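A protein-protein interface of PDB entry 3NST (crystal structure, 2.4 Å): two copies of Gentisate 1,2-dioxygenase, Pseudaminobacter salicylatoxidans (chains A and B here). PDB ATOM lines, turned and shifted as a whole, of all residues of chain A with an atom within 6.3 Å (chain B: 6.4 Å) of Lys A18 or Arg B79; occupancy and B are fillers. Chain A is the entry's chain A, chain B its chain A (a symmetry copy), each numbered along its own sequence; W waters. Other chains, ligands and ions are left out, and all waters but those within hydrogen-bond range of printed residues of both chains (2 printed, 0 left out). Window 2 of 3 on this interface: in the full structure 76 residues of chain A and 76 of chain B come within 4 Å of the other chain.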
ATOM      1  N   MET A  15      15.976   6.090 -13.366  1.00  0.00           N
ATOM      2  CA  MET A  15      17.112   6.394 -12.458  1.00  0.00           C
ATOM      3  C   MET A  15      18.308   5.513 -12.875  1.00  0.00           C
ATOM      4  O   MET A  15      18.133   4.468 -13.509  1.00  0.00           O
ATOM      5  CB  MET A  15      16.717   6.213 -10.960  1.00  0.00           C
ATOM      6  N   GLN A  16      19.512   5.973 -12.540  1.00  0.00           N
ATOM      7  CA  GLN A  16      20.774   5.318 -12.877  1.00  0.00           C
ATOM      8  C   GLN A  16      21.291   4.550 -11.659  1.00  0.00           C
ATOM      9  O   GLN A  16      20.796   4.779 -10.553  1.00  0.00           O
ATOM     10  CB  GLN A  16      21.771   6.420 -13.241  1.00  0.00           C
ATOM     11  CG  GLN A  16      21.546   6.995 -14.641  1.00  0.00           C
ATOM     12  CD  GLN A  16      21.880   5.996 -15.806  1.00  0.00           C
ATOM     13  OE1 GLN A  16      22.932   5.324 -15.806  1.00  0.00           O
ATOM     14  NE2 GLN A  16      20.967   5.894 -16.772  1.00  0.00           N
ATOM     15  N   PRO A  17      22.301   3.658 -11.834  1.00  0.00           N
ATOM     16  CA  PRO A  17      22.899   2.982 -10.655  1.00  0.00           C
ATOM     17  C   PRO A  17      23.586   3.960  -9.692  1.00  0.00           C
ATOM     18  O   PRO A  17      23.913   5.082 -10.087  1.00  0.00           O
ATOM     19  CB  PRO A  17      23.936   2.000 -11.270  1.00  0.00           C
ATOM     20  CG  PRO A  17      24.125   2.432 -12.633  1.00  0.00           C
ATOM     21  CD  PRO A  17      22.876   3.152 -13.093  1.00  0.00           C
ATOM     22  N   LYS A  18      23.780   3.556  -8.442  1.00  0.00           N
ATOM     23  CA  LYS A  18      24.374   4.456  -7.466  1.00  0.00           C
ATOM     24  C   LYS A  18      25.783   4.853  -7.920  1.00  0.00           C
ATOM     25  O   LYS A  18      26.554   3.974  -8.297  1.00  0.00           O
ATOM     26  CB  LYS A  18      24.459   3.746  -6.126  1.00  0.00           C
ATOM     27  CG  LYS A  18      23.133   3.598  -5.401  1.00  0.00           C
ATOM     28  CD  LYS A  18      23.278   2.621  -4.229  1.00  0.00           C
ATOM     29  CE  LYS A  18      21.948   2.388  -3.478  1.00  0.00           C
ATOM     30  NZ  LYS A  18      21.888   1.103  -2.639  1.00  0.00           N
ATOM     31  N   ASP A  19      26.124   6.147  -7.897  1.00  0.00           N
ATOM     32  CA  ASP A  19      27.473   6.639  -8.320  1.00  0.00           C
ATOM     33  C   ASP A  19      28.557   6.510  -7.234  1.00  0.00           C
ATOM     34  O   ASP A  19      28.854   7.422  -6.485  1.00  0.00           O
ATOM     35  CB  ASP A  19      27.394   8.079  -8.806  1.00  0.00           C
ATOM     36  CG  ASP A  19      28.697   8.573  -9.407  1.00  0.00           C
ATOM     37  OD1 ASP A  19      29.605   7.775  -9.697  1.00  0.00           O
ATOM     38  OD2 ASP A  19      28.847   9.793  -9.581  1.00  0.00           O
ATOM     39  N   THR A  20      29.221   5.376  -7.290  1.00  0.00           N
ATOM     40  CA  THR A  20      30.019   4.786  -6.251  1.00  0.00           C
ATOM     41  C   THR A  20      31.469   4.603  -6.774  1.00  0.00           C
ATOM     42  O   THR A  20      31.705   4.688  -7.980  1.00  0.00           O
ATOM     43  CB  THR A  20      29.253   3.505  -5.975  1.00  0.00           C
ATOM     44  OG1 THR A  20      28.427   3.703  -4.813  1.00  0.00           O
ATOM     45  CG2 THR A  20      30.072   2.331  -5.818  1.00  0.00           C
ATOM     46  N   LEU A  23      31.177   1.747  -9.132  1.00  0.00           N
ATOM     47  CA  LEU A  23      30.465   1.963 -10.366  1.00  0.00           C
ATOM     48  C   LEU A  23      31.407   2.661 -11.355  1.00  0.00           C
ATOM     49  O   LEU A  23      31.287   2.438 -12.580  1.00  0.00           O
ATOM     50  CB  LEU A  23      29.161   2.731 -10.173  1.00  0.00           C
ATOM     51  CG  LEU A  23      28.399   2.836 -11.506  1.00  0.00           C
ATOM     52  CD1 LEU A  23      27.739   1.490 -11.915  1.00  0.00           C
ATOM     53  CD2 LEU A  23      27.366   4.021 -11.610  1.00  0.00           C
ATOM     54  N   TRP A  39      22.146   0.779 -20.532  1.00  0.00           N
ATOM     55  CA  TRP A  39      21.308   1.546 -19.572  1.00  0.00           C
ATOM     56  C   TRP A  39      21.692   3.015 -19.435  1.00  0.00           C
ATOM     57  O   TRP A  39      21.128   3.747 -18.611  1.00  0.00           O
ATOM     58  CB  TRP A  39      21.287   0.902 -18.184  1.00  0.00           C
ATOM     59  CG  TRP A  39      22.619   0.871 -17.495  1.00  0.00           C
ATOM     60  CD1 TRP A  39      23.178   1.863 -16.770  1.00  0.00           C
ATOM     61  CD2 TRP A  39      23.574  -0.223 -17.481  1.00  0.00           C
ATOM     62  NE1 TRP A  39      24.438   1.473 -16.302  1.00  0.00           N
ATOM     63  CE2 TRP A  39      24.684   0.192 -16.711  1.00  0.00           C
ATOM     64  CE3 TRP A  39      23.588  -1.499 -18.036  1.00  0.00           C
ATOM     65  CZ2 TRP A  39      25.785  -0.634 -16.471  1.00  0.00           C
ATOM     66  CZ3 TRP A  39      24.685  -2.321 -17.794  1.00  0.00           C
ATOM     67  CH2 TRP A  39      25.752  -1.882 -17.019  1.00  0.00           C
ATOM     68  N   LEU B  74      26.007  -4.257  -9.340  1.00  0.00           N
ATOM     69  CA  LEU B  74      25.965  -2.828  -9.199  1.00  0.00           C
ATOM     70  C   LEU B  74      24.710  -2.235  -9.784  1.00  0.00           C
ATOM     71  O   LEU B  74      24.412  -1.078  -9.501  1.00  0.00           O
ATOM     72  CB  LEU B  74      27.207  -2.175  -9.792  1.00  0.00           C
ATOM     73  CG  LEU B  74      28.500  -2.638  -9.159  1.00  0.00           C
ATOM     74  CD1 LEU B  74      29.649  -1.800  -9.582  1.00  0.00           C
ATOM     75  CD2 LEU B  74      28.377  -2.607  -7.622  1.00  0.00           C
ATOM     76  N   VAL B  75      23.965  -2.978 -10.599  1.00  0.00           N
ATOM     77  CA  VAL B  75      22.950  -2.322 -11.436  1.00  0.00           C
ATOM     78  C   VAL B  75      21.675  -3.095 -11.288  1.00  0.00           C
ATOM     79  O   VAL B  75      21.413  -3.982 -12.082  1.00  0.00           O
ATOM     80  CB  VAL B  75      23.385  -2.275 -12.918  1.00  0.00           C
ATOM     81  CG1 VAL B  75      22.347  -1.607 -13.761  1.00  0.00           C
ATOM     82  CG2 VAL B  75      24.806  -1.581 -13.084  1.00  0.00           C
ATOM     83  N   PRO B  76      20.890  -2.797 -10.227  1.00  0.00           N
ATOM     84  CA  PRO B  76      19.680  -3.601  -9.934  1.00  0.00           C
ATOM     85  C   PRO B  76      18.495  -3.082 -10.739  1.00  0.00           C
ATOM     86  O   PRO B  76      18.587  -1.982 -11.329  1.00  0.00           O
ATOM     87  CB  PRO B  76      19.439  -3.346  -8.426  1.00  0.00           C
ATOM     88  CG  PRO B  76      19.977  -1.897  -8.197  1.00  0.00           C
ATOM     89  CD  PRO B  76      21.081  -1.684  -9.257  1.00  0.00           C
ATOM     90  N   VAL B  77      17.404  -3.859 -10.761  1.00  0.00           N
ATOM     91  CA  VAL B  77      16.169  -3.374 -11.349  1.00  0.00           C
ATOM     92  C   VAL B  77      15.648  -2.134 -10.576  1.00  0.00           C
ATOM     93  O   VAL B  77      15.767  -2.068  -9.344  1.00  0.00           O
ATOM     94  CB  VAL B  77      15.117  -4.481 -11.553  1.00  0.00           C
ATOM     95  CG1 VAL B  77      15.412  -5.226 -12.857  1.00  0.00           C
ATOM     96  CG2 VAL B  77      15.071  -5.455 -10.365  1.00  0.00           C
ATOM     97  N   GLY B  78      15.141  -1.143 -11.319  1.00  0.00           N
ATOM     98  CA  GLY B  78      14.823   0.186 -10.792  1.00  0.00           C
ATOM     99  C   GLY B  78      15.923   1.235 -11.015  1.00  0.00           C
ATOM    100  O   GLY B  78      15.649   2.436 -11.019  1.00  0.00           O
ATOM    101  N   ARG B  79      17.164   0.771 -11.189  1.00  0.00           N
ATOM    102  CA  ARG B  79      18.354   1.639 -11.315  1.00  0.00           C
ATOM    103  C   ARG B  79      19.175   1.270 -12.575  1.00  0.00           C
ATOM    104  O   ARG B  79      20.397   1.305 -12.536  1.00  0.00           O
ATOM    105  CB  ARG B  79      19.268   1.507 -10.067  1.00  0.00           C
ATOM    106  CG  ARG B  79      18.695   2.004  -8.718  1.00  0.00           C
ATOM    107  CD  ARG B  79      18.813   3.523  -8.539  1.00  0.00           C
ATOM    108  NE  ARG B  79      19.175   3.843  -7.165  1.00  0.00           N
ATOM    109  CZ  ARG B  79      19.857   4.914  -6.747  1.00  0.00           C
ATOM    110  NH1 ARG B  79      20.314   5.854  -7.588  1.00  0.00           N
ATOM    111  NH2 ARG B  79      20.111   5.034  -5.442  1.00  0.00           N
ATOM    112  N   GLY B  80      18.495   0.875 -13.652  1.00  0.00           N
ATOM    113  CA  GLY B  80      19.134   0.470 -14.905  1.00  0.00           C
ATOM    114  C   GLY B  80      19.120  -1.033 -15.178  1.00  0.00           C
ATOM    115  O   GLY B  80      19.374  -1.451 -16.313  1.00  0.00           O
ATOM    116  N   GLY B  81      18.818  -1.842 -14.155  1.00  0.00           N
ATOM    117  CA  GLY B  81      18.715  -3.311 -14.261  1.00  0.00           C
ATOM    118  C   GLY B  81      17.801  -3.935 -15.326  1.00  0.00           C
ATOM    119  O   GLY B  81      18.106  -5.027 -15.838  1.00  0.00           O
ATOM    120  N   GLU B  82      16.683  -3.252 -15.646  1.00  0.00           N
ATOM    121  CA  GLU B  82      15.769  -3.607 -16.784  1.00  0.00           C
ATOM    122  C   GLU B  82      16.558  -3.640 -18.129  1.00  0.00           C
ATOM    123  O   GLU B  82      16.180  -4.396 -19.060  1.00  0.00           O
ATOM    124  CB  GLU B  82      14.615  -2.578 -17.014  1.00  0.00           C
ATOM    125  CG  GLU B  82      13.836  -1.955 -15.826  1.00  0.00           C
ATOM    126  CD  GLU B  82      14.718  -1.295 -14.721  1.00  0.00           C
ATOM    127  OE1 GLU B  82      14.643  -1.795 -13.587  1.00  0.00           O
ATOM    128  OE2 GLU B  82      15.474  -0.317 -14.948  1.00  0.00           O
HETATM  129  O   HOH W   1      22.824   1.037  -7.966  1.00  0.00           O
HETATM  130  O   HOH W   2      26.456   1.274  -7.935  1.00  0.00           O
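Water W2 bridges the backbone carbonyl oxygen of Lys A18 and the backbone carbonyl oxygen of Leu B74. Water W1 bridges N of Lys A18 and O of Leu B74.
The guanidinium group (NH1) of Arg B79 sits close to the backbone carbonyl oxygen (O) of Gln A16. The backbone nitrogen (N) of Pro A17 sits close to the backbone carbonyl oxygen (O) of Arg B79, at 3.1 Å.
N of Gly B80 is in hydrogen-bond range of OE2 of Glu B82. The side-chain amide nitrogen (NE2) of Gln A16 is in hydrogen-bond range of the backbone carbonyl oxygen (O) of Trp A39 (2.8 Å). The backbone NH (N) of Gly B78 sits at hydrogen-bond distance from the side-chain carboxylate (OE1) of Glu B82, at 2.4 Å.
Hydrophobic or aromatic side chains of chain B within 4 Å of the printed part of chain A: Leu B74 and Val B75. Hydrophobic or aromatic side chains of chain A that line the printed part of chain B: Met A15, Pro A17 and Trp A39. Among the printed residues, 10 pairs touch across the chains. Among the printed residues, no Asp or Glu carboxylate lies within 4 Å of a Lys or Arg side-chain nitrogen of the other chain.
Gly B78 touches Met A15 (O to CB, 3.9 Å). O of Met A15 touches C of Arg B79, at 3.5 Å. N of Gly B80 touches O of Met A15 (3.6 Å). Leu B74 touches Pro A17 (O to CB, 3.6 Å). Lys A18 touches Arg B79. Leu A23 touches Leu B74 (N to CD1, 3.9 Å). CZ2 of Trp A39 touches CG2 of Val B75 (3.7 Å). Trp A39 touches Gly B80 (CB to O, 3.6 Å).
Of the printed residues of chain B, Gln A16 touches Arg B79 (3.1 Å). Of the printed residues of chain B, Pro A17 touches Leu B74 (3.6 Å) and Arg B79 (3.1 Å). Lys A18 touches just one residue of chain B: Arg B79 (3.3 Å). Of the printed residues of chain B, Leu A23 touches Leu B74. Val B77 touches none of the printed residues of chain A. Printed residues of chain A within 4 Å of Gly B78: Met A15. Of chain A, only Met A15, Gln A16, Pro A17 and Lys A18 come within 4 Å of Arg B79.
No position is printed for both chains. Of the 10 pairs that touch across the chains among the printed residues, none has its exchanged pair printed and touching as well.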
